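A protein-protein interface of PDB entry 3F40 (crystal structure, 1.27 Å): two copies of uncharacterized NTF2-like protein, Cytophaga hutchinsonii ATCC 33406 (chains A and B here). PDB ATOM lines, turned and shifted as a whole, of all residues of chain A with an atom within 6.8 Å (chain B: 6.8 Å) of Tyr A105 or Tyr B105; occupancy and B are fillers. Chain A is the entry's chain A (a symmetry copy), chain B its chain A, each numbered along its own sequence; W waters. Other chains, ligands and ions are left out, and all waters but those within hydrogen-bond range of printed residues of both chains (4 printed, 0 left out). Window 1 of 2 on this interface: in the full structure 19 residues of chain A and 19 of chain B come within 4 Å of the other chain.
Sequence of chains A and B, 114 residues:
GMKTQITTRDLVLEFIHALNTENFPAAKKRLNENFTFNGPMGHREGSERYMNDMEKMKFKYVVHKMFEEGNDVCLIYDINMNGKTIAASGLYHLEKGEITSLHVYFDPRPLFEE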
ATOM      1  N   ASN A  38     -11.201  26.164  14.122  1.00  0.00           N
ATOM      2  CA  ASN A  38     -12.427  25.808  13.428  1.00  0.00           C
ATOM      3  C   ASN A  38     -12.961  24.519  13.968  1.00  0.00           C
ATOM      4  O   ASN A  38     -12.265  23.520  14.036  1.00  0.00           O
ATOM      5  CB  ASN A  38     -12.198  25.642  11.966  1.00  0.00           C
ATOM      6  CG  ASN A  38     -12.123  26.900  11.283  1.00  0.00           C
ATOM      7  OD1 ASN A  38     -13.137  27.403  10.708  1.00  0.00           O
ATOM      8  ND2 ASN A  38     -10.965  27.464  11.288  1.00  0.00           N
ATOM      9  N   GLY A  39     -14.224  24.549  14.338  1.00  0.00           N
ATOM     10  CA  GLY A  39     -14.912  23.369  14.802  1.00  0.00           C
ATOM     11  C   GLY A  39     -16.339  23.390  14.313  1.00  0.00           C
ATOM     12  O   GLY A  39     -16.770  24.364  13.660  1.00  0.00           O
ATOM     13  N   PRO A  40     -17.096  22.350  14.651  1.00  0.00           N
ATOM     14  CA  PRO A  40     -18.491  22.284  14.195  1.00  0.00           C
ATOM     15  C   PRO A  40     -19.343  23.481  14.602  1.00  0.00           C
ATOM     16  O   PRO A  40     -20.333  23.851  13.921  1.00  0.00           O
ATOM     17  CB  PRO A  40     -19.020  21.052  14.909  1.00  0.00           C
ATOM     18  CG  PRO A  40     -17.876  20.248  15.259  1.00  0.00           C
ATOM     19  CD  PRO A  40     -16.663  21.132  15.349  1.00  0.00           C
ATOM     20  N   CYS A  74      -2.421  14.951  13.466  1.00  0.00           N
ATOM     21  CA  CYS A  74      -3.830  14.627  13.669  1.00  0.00           C
ATOM     22  C   CYS A  74      -4.012  13.677  14.840  1.00  0.00           C
ATOM     23  O   CYS A  74      -3.444  12.589  14.872  1.00  0.00           O
ATOM     24  CB  CYS A  74      -4.453  14.037  12.396  1.00  0.00           C
ATOM     25  SG  CYS A  74      -6.268  14.104  12.417  1.00  0.00           S
ATOM     26  N   ILE A  76      -6.685  11.466  17.218  1.00  0.00           N
ATOM     27  CA  ILE A  76      -7.945  10.803  17.420  1.00  0.00           C
ATOM     28  C   ILE A  76      -8.121  10.750  18.928  1.00  0.00           C
ATOM     29  O   ILE A  76      -7.336  10.138  19.643  1.00  0.00           O
ATOM     30  CB  ILE A  76      -7.934   9.378  16.842  1.00  0.00           C
ATOM     31  CG1 ILE A  76      -7.623   9.391  15.346  1.00  0.00           C
ATOM     32  CG2 ILE A  76      -9.244   8.651  17.098  1.00  0.00           C
ATOM     33  CD1 ILE A  76      -8.603  10.172  14.490  1.00  0.00           C
ATOM     34  N   TYR A  77      -9.136  11.451  19.409  1.00  0.00           N
ATOM     35  CA  TYR A  77      -9.319  11.593  20.830  1.00  0.00           C
ATOM     36  C   TYR A  77     -10.777  11.717  21.237  1.00  0.00           C
ATOM     37  O   TYR A  77     -11.635  12.139  20.474  1.00  0.00           O
ATOM     38  CB  TYR A  77      -8.489  12.761  21.380  1.00  0.00           C
ATOM     39  CG  TYR A  77      -8.547  14.155  20.719  1.00  0.00           C
ATOM     40  CD1 TYR A  77      -9.534  14.538  19.835  1.00  0.00           C
ATOM     41  CD2 TYR A  77      -7.596  15.093  21.056  1.00  0.00           C
ATOM     42  CE1 TYR A  77      -9.530  15.814  19.257  1.00  0.00           C
ATOM     43  CE2 TYR A  77      -7.571  16.361  20.521  1.00  0.00           C
ATOM     44  CZ  TYR A  77      -8.541  16.726  19.613  1.00  0.00           C
ATOM     45  OH  TYR A  77      -8.526  18.008  19.069  1.00  0.00           O
ATOM     46  N   ASP A  78     -11.031  11.332  22.490  1.00  0.00           N
ATOM     47  CA  ASP A  78     -12.334  11.542  23.106  1.00  0.00           C
ATOM     48  C   ASP A  78     -12.231  12.866  23.850  1.00  0.00           C
ATOM     49  O   ASP A  78     -11.256  13.105  24.598  1.00  0.00           O
ATOM     50  CB  ASP A  78     -12.707  10.412  24.048  1.00  0.00           C
ATOM     51  CG  ASP A  78     -13.038   9.133  23.331  1.00  0.00           C
ATOM     52  OD1 ASP A  78     -13.337   9.134  22.126  1.00  0.00           O
ATOM     53  OD2 ASP A  78     -13.033   8.095  24.015  1.00  0.00           O
ATOM     54  N   ILE A  79     -13.230  13.727  23.668  1.00  0.00           N
ATOM     55  CA  ILE A  79     -13.268  15.006  24.351  1.00  0.00           C
ATOM     56  C   ILE A  79     -14.463  15.024  25.299  1.00  0.00           C
ATOM     57  O   ILE A  79     -15.599  14.766  24.907  1.00  0.00           O
ATOM     58  CB  ILE A  79     -13.374  16.223  23.389  1.00  0.00           C
ATOM     59  CG1 ILE A  79     -12.443  16.099  22.170  1.00  0.00           C
ATOM     60  CG2 ILE A  79     -13.070  17.487  24.172  1.00  0.00           C
ATOM     61  CD1 ILE A  79     -12.631  17.210  21.157  1.00  0.00           C
ATOM     62  N   ILE A  86     -17.377  12.985  23.532  1.00  0.00           N
ATOM     63  CA  ILE A  86     -17.509  13.023  22.094  1.00  0.00           C
ATOM     64  C   ILE A  86     -16.240  12.532  21.452  1.00  0.00           C
ATOM     65  O   ILE A  86     -15.160  12.987  21.809  1.00  0.00           O
ATOM     66  CB  ILE A  86     -17.723  14.477  21.649  1.00  0.00           C
ATOM     67  CG1 ILE A  86     -18.985  15.042  22.314  1.00  0.00           C
ATOM     68  CG2 ILE A  86     -17.717  14.606  20.105  1.00  0.00           C
ATOM     69  CD1 ILE A  86     -20.250  14.737  21.603  1.00  0.00           C
ATOM     70  N   ALA A  87     -16.378  11.596  20.511  1.00  0.00           N
ATOM     71  CA  ALA A  87     -15.241  11.121  19.738  1.00  0.00           C
ATOM     72  C   ALA A  87     -14.983  12.103  18.615  1.00  0.00           C
ATOM     73  O   ALA A  87     -15.860  12.395  17.809  1.00  0.00           O
ATOM     74  CB  ALA A  87     -15.473   9.714  19.165  1.00  0.00           C
ATOM     75  N   ALA A  88     -13.737  12.550  18.533  1.00  0.00           N
ATOM     76  CA  ALA A  88     -13.339  13.574  17.571  1.00  0.00           C
ATOM     77  C   ALA A  88     -11.992  13.266  16.939  1.00  0.00           C
ATOM     78  O   ALA A  88     -11.220  12.434  17.414  1.00  0.00           O
ATOM     79  CB  ALA A  88     -13.231  14.952  18.280  1.00  0.00           C
ATOM     80  N   SER A  89     -11.739  13.982  15.858  1.00  0.00           N
ATOM     81  CA  SER A  89     -10.444  14.025  15.207  1.00  0.00           C
ATOM     82  C   SER A  89      -9.990  15.484  15.181  1.00  0.00           C
ATOM     83  O   SER A  89     -10.731  16.323  14.740  1.00  0.00           O
ATOM     84  CB  SER A  89     -10.550  13.470  13.785  1.00  0.00           C
ATOM     85  OG  SER A  89      -9.305  13.542  13.129  1.00  0.00           O
ATOM     86  N   GLY A  90      -8.779  15.758  15.635  1.00  0.00           N
ATOM     87  CA  GLY A  90      -8.258  17.119  15.698  1.00  0.00           C
ATOM     88  C   GLY A  90      -7.031  17.238  14.825  1.00  0.00           C
ATOM     89  O   GLY A  90      -6.065  16.490  14.975  1.00  0.00           O
ATOM     90  N   LEU A  91      -7.068  18.199  13.903  1.00  0.00           N
ATOM     91  CA  LEU A  91      -5.995  18.450  12.952  1.00  0.00           C
ATOM     92  C   LEU A  91      -5.281  19.747  13.338  1.00  0.00           C
ATOM     93  O   LEU A  91      -5.855  20.834  13.290  1.00  0.00           O
ATOM     94  CB  LEU A  91      -6.577  18.572  11.555  1.00  0.00           C
ATOM     95  CG  LEU A  91      -5.618  18.924  10.440  1.00  0.00           C
ATOM     96  CD1 LEU A  91      -4.590  17.819  10.202  1.00  0.00           C
ATOM     97  CD2 LEU A  91      -6.422  19.222   9.163  1.00  0.00           C
ATOM     98  N   HIS A 103      -8.308  22.426  13.425  1.00  0.00           N
ATOM     99  CA  HIS A 103      -9.588  22.090  12.870  1.00  0.00           C
ATOM    100  C   HIS A 103     -10.043  20.803  13.534  1.00  0.00           C
ATOM    101  O   HIS A 103      -9.328  19.808  13.435  1.00  0.00           O
ATOM    102  CB  HIS A 103      -9.463  21.832  11.373  1.00  0.00           C
ATOM    103  CG  HIS A 103      -9.200  23.048  10.574  1.00  0.00           C
ATOM    104  ND1 HIS A 103      -7.970  23.674  10.563  1.00  0.00           N
ATOM    105  CD2 HIS A 103      -9.998  23.755   9.741  1.00  0.00           C
ATOM    106  CE1 HIS A 103      -8.033  24.735   9.763  1.00  0.00           C
ATOM    107  NE2 HIS A 103      -9.257  24.804   9.257  1.00  0.00           N
ATOM    108  N   VAL A 104     -11.168  20.847  14.244  1.00  0.00           N
ATOM    109  CA  VAL A 104     -11.655  19.658  14.955  1.00  0.00           C
ATOM    110  C   VAL A 104     -12.953  19.177  14.310  1.00  0.00           C
ATOM    111  O   VAL A 104     -13.804  19.961  13.922  1.00  0.00           O
ATOM    112  CB  VAL A 104     -11.770  19.919  16.500  1.00  0.00           C
ATOM    113  CG1 VAL A 104     -12.824  20.922  16.832  1.00  0.00           C
ATOM    114  CG2 VAL A 104     -11.977  18.613  17.241  1.00  0.00           C
ATOM    115  N   TYR A 105     -13.036  17.869  14.187  1.00  0.00           N
ATOM    116  CA  TYR A 105     -14.105  17.176  13.468  1.00  0.00           C
ATOM    117  C   TYR A 105     -14.876  16.272  14.407  1.00  0.00           C
ATOM    118  O   TYR A 105     -14.299  15.370  14.982  1.00  0.00           O
ATOM    119  CB  TYR A 105     -13.538  16.314  12.339  1.00  0.00           C
ATOM    120  CG  TYR A 105     -12.720  17.017  11.312  1.00  0.00           C
ATOM    121  CD1 TYR A 105     -11.391  17.297  11.538  1.00  0.00           C
ATOM    122  CD2 TYR A 105     -13.269  17.367  10.095  1.00  0.00           C
ATOM    123  CE1 TYR A 105     -10.629  17.928  10.571  1.00  0.00           C
ATOM    124  CE2 TYR A 105     -12.523  17.967   9.128  1.00  0.00           C
ATOM    125  CZ  TYR A 105     -11.191  18.269   9.380  1.00  0.00           C
ATOM    126  OH  TYR A 105     -10.418  18.842   8.399  1.00  0.00           O
ATOM    127  N   PHE A 106     -16.175  16.490  14.497  1.00  0.00           N
ATOM    128  CA  PHE A 106     -17.060  15.655  15.274  1.00  0.00           C
ATOM    129  C   PHE A 106     -18.505  16.025  15.036  1.00  0.00           C
ATOM    130  O   PHE A 106     -18.793  17.088  14.493  1.00  0.00           O
ATOM    131  CB  PHE A 106     -16.753  15.690  16.789  1.00  0.00           C
ATOM    132  CG  PHE A 106     -16.909  17.041  17.462  1.00  0.00           C
ATOM    133  CD1 PHE A 106     -15.831  17.880  17.574  1.00  0.00           C
ATOM    134  CD2 PHE A 106     -18.108  17.397  18.078  1.00  0.00           C
ATOM    135  CE1 PHE A 106     -15.937  19.083  18.228  1.00  0.00           C
ATOM    136  CE2 PHE A 106     -18.205  18.621  18.710  1.00  0.00           C
ATOM    137  CZ  PHE A 106     -17.116  19.444  18.793  1.00  0.00           C
ATOM    138  N   ASP A 107     -19.389  15.129  15.456  1.00  0.00           N
ATOM    139  CA  ASP A 107     -20.834  15.365  15.392  1.00  0.00           C
ATOM    140  C   ASP A 107     -21.265  16.050  16.696  1.00  0.00           C
ATOM    141  O   ASP A 107     -21.215  15.436  17.765  1.00  0.00           O
ATOM    142  CB  ASP A 107     -21.566  14.039  15.215  1.00  0.00           C
ATOM    143  CG  ASP A 107     -23.070  14.162  15.294  1.00  0.00           C
ATOM    144  OD1 ASP A 107     -23.603  15.284  15.370  1.00  0.00           O
ATOM    145  OD2 ASP A 107     -23.703  13.064  15.288  1.00  0.00           O
ATOM    146  N   ASN B  38     -18.570   3.261  11.067  1.00  0.00           N
ATOM    147  CA  ASN B  38     -19.156   4.163  12.044  1.00  0.00           C
ATOM    148  C   ASN B  38     -19.035   5.576  11.569  1.00  0.00           C
ATOM    149  O   ASN B  38     -17.963   6.042  11.225  1.00  0.00           O
ATOM    150  CB  ASN B  38     -18.476   4.055  13.364  1.00  0.00           C
ATOM    151  CG  ASN B  38     -18.905   2.903  14.103  1.00  0.00           C
ATOM    152  OD1 ASN B  38     -19.821   2.981  14.978  1.00  0.00           O
ATOM    153  ND2 ASN B  38     -18.292   1.807  13.822  1.00  0.00           N
ATOM    154  N   GLY B  39     -20.158   6.263  11.571  1.00  0.00           N
ATOM    155  CA  GLY B  39     -20.198   7.662  11.220  1.00  0.00           C
ATOM    156  C   GLY B  39     -21.205   8.374  12.089  1.00  0.00           C
ATOM    157  O   GLY B  39     -21.890   7.736  12.915  1.00  0.00           O
ATOM    158  N   PRO B  40     -21.339   9.682  11.889  1.00  0.00           N
ATOM    159  CA  PRO B  40     -22.283  10.452  12.711  1.00  0.00           C
ATOM    160  C   PRO B  40     -23.720   9.944  12.660  1.00  0.00           C
ATOM    161  O   PRO B  40     -24.515  10.111  13.620  1.00  0.00           O
ATOM    162  CB  PRO B  40     -22.238  11.830  12.072  1.00  0.00           C
ATOM    163  CG  PRO B  40     -20.994  11.915  11.349  1.00  0.00           C
ATOM    164  CD  PRO B  40     -20.533  10.527  10.999  1.00  0.00           C
ATOM    165  N   CYS B  74      -5.362   7.857   8.294  1.00  0.00           N
ATOM    166  CA  CYS B  74      -6.363   8.906   8.467  1.00  0.00           C
ATOM    167  C   CYS B  74      -6.322   9.898   7.319  1.00  0.00           C
ATOM    168  O   CYS B  74      -5.293  10.506   7.037  1.00  0.00           O
ATOM    169  CB  CYS B  74      -6.183   9.629   9.809  1.00  0.00           C
ATOM    170  SG  CYS B  74      -7.666  10.555  10.303  1.00  0.00           S
ATOM    171  N   ILE B  76      -7.917  13.393   5.606  1.00  0.00           N
ATOM    172  CA  ILE B  76      -8.615  14.646   5.709  1.00  0.00           C
ATOM    173  C   ILE B  76      -9.148  14.913   4.312  1.00  0.00           C
ATOM    174  O   ILE B  76      -8.394  15.062   3.357  1.00  0.00           O
ATOM    175  CB  ILE B  76      -7.675  15.785   6.139  1.00  0.00           C
ATOM    176  CG1 ILE B  76      -7.017  15.480   7.484  1.00  0.00           C
ATOM    177  CG2 ILE B  76      -8.394  17.123   6.199  1.00  0.00           C
ATOM    178  CD1 ILE B  76      -7.977  15.283   8.642  1.00  0.00           C
ATOM    179  N   TYR B  77     -10.467  14.913   4.195  1.00  0.00           N
ATOM    180  CA  TYR B  77     -11.087  15.013   2.899  1.00  0.00           C
ATOM    181  C   TYR B  77     -12.424  15.731   2.928  1.00  0.00           C
ATOM    182  O   TYR B  77     -13.120  15.776   3.934  1.00  0.00           O
ATOM    183  CB  TYR B  77     -11.212  13.634   2.239  1.00  0.00           C
ATOM    184  CG  TYR B  77     -11.825  12.441   3.005  1.00  0.00           C
ATOM    185  CD1 TYR B  77     -12.569  12.579   4.158  1.00  0.00           C
ATOM    186  CD2 TYR B  77     -11.671  11.171   2.495  1.00  0.00           C
ATOM    187  CE1 TYR B  77     -13.092  11.459   4.818  1.00  0.00           C
ATOM    188  CE2 TYR B  77     -12.185  10.050   3.107  1.00  0.00           C
ATOM    189  CZ  TYR B  77     -12.899  10.192   4.277  1.00  0.00           C
ATOM    190  OH  TYR B  77     -13.427   9.064   4.902  1.00  0.00           O
ATOM    191  N   ASP B  78     -12.769  16.296   1.768  1.00  0.00           N
ATOM    192  CA  ASP B  78     -14.089  16.875   1.562  1.00  0.00           C
ATOM    193  C   ASP B  78     -14.931  15.773   0.933  1.00  0.00           C
ATOM    194  O   ASP B  78     -14.495  15.110  -0.036  1.00  0.00           O
ATOM    195  CB  ASP B  78     -14.038  18.103   0.670  1.00  0.00           C
ATOM    196  CG  ASP B  78     -13.410  19.292   1.340  1.00  0.00           C
ATOM    197  OD1 ASP B  78     -13.311  19.351   2.577  1.00  0.00           O
ATOM    198  OD2 ASP B  78     -13.038  20.216   0.598  1.00  0.00           O
ATOM    199  N   ILE B  79     -16.137  15.576   1.459  1.00  0.00           N
ATOM    200  CA  ILE B  79     -17.049  14.583   0.924  1.00  0.00           C
ATOM    201  C   ILE B  79     -18.273  15.293   0.353  1.00  0.00           C
ATOM    202  O   ILE B  79     -18.926  16.089   1.024  1.00  0.00           O
ATOM    203  CB  ILE B  79     -17.521  13.540   1.976  1.00  0.00           C
ATOM    204  CG1 ILE B  79     -16.374  13.038   2.871  1.00  0.00           C
ATOM    205  CG2 ILE B  79     -18.181  12.384   1.248  1.00  0.00           C
ATOM    206  CD1 ILE B  79     -16.840  12.124   3.986  1.00  0.00           C
ATOM    207  N   ILE B  86     -18.991  18.425   2.686  1.00  0.00           N
ATOM    208  CA  ILE B  86     -18.714  18.343   4.102  1.00  0.00           C
ATOM    209  C   ILE B  86     -17.262  18.015   4.319  1.00  0.00           C
ATOM    210  O   ILE B  86     -16.750  17.081   3.714  1.00  0.00           O
ATOM    211  CB  ILE B  86     -19.545  17.203   4.709  1.00  0.00           C
ATOM    212  CG1 ILE B  86     -21.037  17.468   4.475  1.00  0.00           C
ATOM    213  CG2 ILE B  86     -19.177  16.962   6.195  1.00  0.00           C
ATOM    214  CD1 ILE B  86     -21.677  18.346   5.482  1.00  0.00           C
ATOM    215  N   ALA B  87     -16.603  18.795   5.179  1.00  0.00           N
ATOM    216  CA  ALA B  87     -15.227  18.514   5.560  1.00  0.00           C
ATOM    217  C   ALA B  87     -15.238  17.457   6.645  1.00  0.00           C
ATOM    218  O   ALA B  87     -15.867  17.619   7.686  1.00  0.00           O
ATOM    219  CB  ALA B  87     -14.492  19.770   6.055  1.00  0.00           C
ATOM    220  N   ALA B  88     -14.468  16.403   6.412  1.00  0.00           N
ATOM    221  CA  ALA B  88     -14.435  15.250   7.307  1.00  0.00           C
ATOM    222  C   ALA B  88     -13.022  14.728   7.509  1.00  0.00           C
ATOM    223  O   ALA B  88     -12.093  15.048   6.768  1.00  0.00           O
ATOM    224  CB  ALA B  88     -15.292  14.098   6.715  1.00  0.00           C
ATOM    225  N   SER B  89     -12.906  13.900   8.532  1.00  0.00           N
ATOM    226  CA  SER B  89     -11.719  13.110   8.796  1.00  0.00           C
ATOM    227  C   SER B  89     -12.139  11.641   8.817  1.00  0.00           C
ATOM    228  O   SER B  89     -13.057  11.302   9.517  1.00  0.00           O
ATOM    229  CB  SER B  89     -11.106  13.513  10.139  1.00  0.00           C
ATOM    230  OG  SER B  89      -9.973  12.725  10.424  1.00  0.00           O
ATOM    231  N   GLY B  90     -11.452  10.796   8.067  1.00  0.00           N
ATOM    232  CA  GLY B  90     -11.791   9.381   7.975  1.00  0.00           C
ATOM    233  C   GLY B  90     -10.637   8.545   8.477  1.00  0.00           C
ATOM    234  O   GLY B  90      -9.509   8.662   8.000  1.00  0.00           O
ATOM    235  N   LEU B  91     -10.928   7.682   9.450  1.00  0.00           N
ATOM    236  CA  LEU B  91      -9.945   6.812  10.081  1.00  0.00           C
ATOM    237  C   LEU B  91     -10.186   5.374   9.620  1.00  0.00           C
ATOM    238  O   LEU B  91     -11.215   4.769   9.918  1.00  0.00           O
ATOM    239  CB  LEU B  91     -10.082   6.907  11.590  1.00  0.00           C
ATOM    240  CG  LEU B  91      -9.198   6.000  12.417  1.00  0.00           C
ATOM    241  CD1 LEU B  91      -7.720   6.351  12.264  1.00  0.00           C
ATOM    242  CD2 LEU B  91      -9.640   6.077  13.889  1.00  0.00           C
ATOM    243  N   HIS B 103     -14.060   4.771  10.610  1.00  0.00           N
ATOM    244  CA  HIS B 103     -14.740   5.696  11.470  1.00  0.00           C
ATOM    245  C   HIS B 103     -14.592   7.076  10.854  1.00  0.00           C
ATOM    246  O   HIS B 103     -13.459   7.515  10.665  1.00  0.00           O
ATOM    247  CB  HIS B 103     -14.082   5.719  12.845  1.00  0.00           C
ATOM    248  CG  HIS B 103     -14.306   4.492  13.638  1.00  0.00           C
ATOM    249  ND1 HIS B 103     -13.665   3.302  13.358  1.00  0.00           N
ATOM    250  CD2 HIS B 103     -15.088   4.260  14.718  1.00  0.00           C
ATOM    251  CE1 HIS B 103     -14.064   2.381  14.230  1.00  0.00           C
ATOM    252  NE2 HIS B 103     -14.931   2.940  15.062  1.00  0.00           N
ATOM    253  N   VAL B 104     -15.708   7.706  10.494  1.00  0.00           N
ATOM    254  CA  VAL B 104     -15.651   9.025   9.850  1.00  0.00           C
ATOM    255  C   VAL B 104     -16.241  10.074  10.790  1.00  0.00           C
ATOM    256  O   VAL B 104     -17.232   9.844  11.465  1.00  0.00           O
ATOM    257  CB  VAL B 104     -16.315   8.999   8.426  1.00  0.00           C
ATOM    258  CG1 VAL B 104     -17.787   8.756   8.488  1.00  0.00           C
ATOM    259  CG2 VAL B 104     -15.982  10.267   7.666  1.00  0.00           C
ATOM    260  N   TYR B 105     -15.567  11.204  10.820  1.00  0.00           N
ATOM    261  CA  TYR B 105     -15.840  12.301  11.749  1.00  0.00           C
ATOM    262  C   TYR B 105     -16.227  13.554  10.990  1.00  0.00           C
ATOM    263  O   TYR B 105     -15.443  14.046  10.203  1.00  0.00           O
ATOM    264  CB  TYR B 105     -14.609  12.622  12.597  1.00  0.00           C
ATOM    265  CG  TYR B 105     -14.052  11.505  13.410  1.00  0.00           C
ATOM    266  CD1 TYR B 105     -13.210  10.572  12.846  1.00  0.00           C
ATOM    267  CD2 TYR B 105     -14.336  11.406  14.757  1.00  0.00           C
ATOM    268  CE1 TYR B 105     -12.676   9.551  13.610  1.00  0.00           C
ATOM    269  CE2 TYR B 105     -13.797  10.419  15.523  1.00  0.00           C
ATOM    270  CZ  TYR B 105     -12.973   9.469  14.935  1.00  0.00           C
ATOM    271  OH  TYR B 105     -12.395   8.489  15.705  1.00  0.00           O
ATOM    272  N   PHE B 106     -17.401  14.080  11.286  1.00  0.00           N
ATOM    273  CA  PHE B 106     -17.870  15.323  10.720  1.00  0.00           C
ATOM    274  C   PHE B 106     -19.151  15.772  11.383  1.00  0.00           C
ATOM    275  O   PHE B 106     -19.801  14.992  12.073  1.00  0.00           O
ATOM    276  CB  PHE B 106     -18.069  15.255   9.189  1.00  0.00           C
ATOM    277  CG  PHE B 106     -19.110  14.265   8.702  1.00  0.00           C
ATOM    278  CD1 PHE B 106     -18.739  12.989   8.364  1.00  0.00           C
ATOM    279  CD2 PHE B 106     -20.427  14.665   8.478  1.00  0.00           C
ATOM    280  CE1 PHE B 106     -19.656  12.094   7.869  1.00  0.00           C
ATOM    281  CE2 PHE B 106     -21.341  13.746   8.004  1.00  0.00           C
ATOM    282  CZ  PHE B 106     -20.945  12.476   7.689  1.00  0.00           C
ATOM    283  N   ASP B 107     -19.486  17.036  11.154  1.00  0.00           N
ATOM    284  CA  ASP B 107     -20.743  17.612  11.639  1.00  0.00           C
ATOM    285  C   ASP B 107     -21.819  17.381  10.570  1.00  0.00           C
ATOM    286  O   ASP B 107     -21.748  17.959   9.482  1.00  0.00           O
ATOM    287  CB  ASP B 107     -20.558  19.104  11.902  1.00  0.00           C
ATOM    288  CG  ASP B 107     -21.842  19.819  12.257  1.00  0.00           C
ATOM    289  OD1 ASP B 107     -22.891  19.173  12.428  1.00  0.00           O
ATOM    290  OD2 ASP B 107     -21.749  21.080  12.347  1.00  0.00           O
HETATM  291  O   HOH W   1     -11.534  17.801   6.068  1.00  0.00           O
HETATM  292  O   HOH W   2     -12.066   9.766  18.159  1.00  0.00           O
HETATM  293  O   HOH W   3     -16.731  18.768  12.278  1.00  0.00           O
HETATM  294  O   HOH W   4     -18.451  12.285  13.755  1.00  0.00           O
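Tyr B105 touches Ile A76 (OH to CG2, 3.4 Å).
Ala A87 touches Tyr B105 (O to CD2, 3.6 Å).
Tyr B105 touches Ala A88.
Tyr B105 touches Ser A89.
Tyr A105 touches Ile B76 (OH to CG2, 3.4 Å).
Ala B87 touches Tyr A105.
Ala B88 touches Tyr A105.
Tyr A105 touches Ser B89 (CD2 to N, 3.8 Å).
CB of Tyr A105 touches O of Tyr B105, 3.7 Å away.
Ile A76 touches Tyr B105, and with the chains exchanged Tyr A105 touches Ile B76.
Ala A88 touches Tyr B105, and with the chains exchanged Tyr A105 touches Ala B88.
Ser A89 touches Tyr B105, and with the chains exchanged Tyr A105 touches Ser B89.
Phe A106 touches its own counterpart, Phe B106.
Of the 15 pairs that touch across the chains among the printed residues, 15 have their exchanged pair printed and touching as well.
The side-chain hydroxyl (OG) of Ser B89 is in hydrogen-bond range of the side-chain sulfur (SG) of Cys B74 (3.2 Å).
N of Ala B88 sits at hydrogen-bond distance from O of Tyr B77.
The backbone carbonyl oxygen (O) of Ser B89 lies within hydrogen-bond range of the backbone NH (N) of Tyr B105, 2.8 Å away.
SG of Cys A74 lies within hydrogen-bond range of OG of Ser A89, at 3.2 Å.
N of Ala A88 is in hydrogen-bond range of O of Tyr A77, at 2.9 Å.
The backbone NH (N) of Tyr A105 sits at hydrogen-bond distance from the backbone carbonyl oxygen (O) of Ser A89, at 2.8 Å.
OG of Ser B89 sits at hydrogen-bond distance from OG of Ser A89, 2.9 Å away.
O of Phe B106 sits at hydrogen-bond distance from N of Asp A107, at 3.4 Å.
The backbone carbonyl oxygen of Phe A106 sits at hydrogen-bond distance from the backbone NH of Asp B107, at 3.4 Å.
The backbone carbonyl oxygen of Pro A40 sits close to the side-chain carboxylate of Asp B107 (3.5 Å).
The backbone carbonyl oxygen (O) of Phe A106 lies close to the backbone carbonyl oxygen (O) of Phe B106, 3.4 Å away.
The side-chain carboxylate (OD2) of Asp A107 sits close to the backbone carbonyl oxygen (O) of Pro B40 (3.5 Å).
Water W2 lies within hydrogen-bond range of OH of Tyr B105 (2.8 Å), O of Ala A88 (2.9 Å) and O of Tyr A77 (3.3 Å).
Water W1 lies within hydrogen-bond range of the side-chain hydroxyl (OH) of Tyr A105, the backbone carbonyl oxygen (O) of Ala B88 and the backbone carbonyl oxygen (O) of Tyr B77.
Water W3 bridges N of Phe A106 (3.2 Å) and N of Asp B107 (3.4 Å).
Water W4 lies within hydrogen-bond range of N of Phe B106 (3.2 Å) and N of Asp A107 (3.4 Å).
Hydrophobic or aromatic side chains of chain B within 4 Å of the printed part of chain A: Pro B40, Ile B76 and Tyr B105.
Printed residues of chain A that touch a printed residue of chain B: Pro A40, Ile A76, Ala A87, Ala A88, Ser A89, Tyr A105, Phe A106 and Asp A107.
Hydrophobic or aromatic side chains of chain A within 4 Å of the printed part of chain B: Pro A40, Ile A76 and Tyr A105.
Among the printed residues, 15 pairs touch across the chains.
Of the printed residues of chain B, Ala A88 touches Tyr B105.
Of chain B, only Ile B76, Ala B87, Ala B88, Ser B89 and Tyr B105 come within 4 Å of Tyr A105.
Of the printed residues of chain A, Ala B87 touches Tyr A105 (3.6 Å).
Of chain A, only Ile A76 (3.4 Å), Ala A87 (3.6 Å), Ala A88 (3.7 Å), Ser A89 (3.8 Å) and Tyr A105 (3.7 Å) come within 4 Å of Tyr B105.
Of the printed residues of chain A, Phe B106 touches Phe A106 (3.4 Å) and Asp A107 (3.4 Å).
The nearest printed residue of chain A that does not touch Ile B76 is Leu A91 (4.1 Å).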
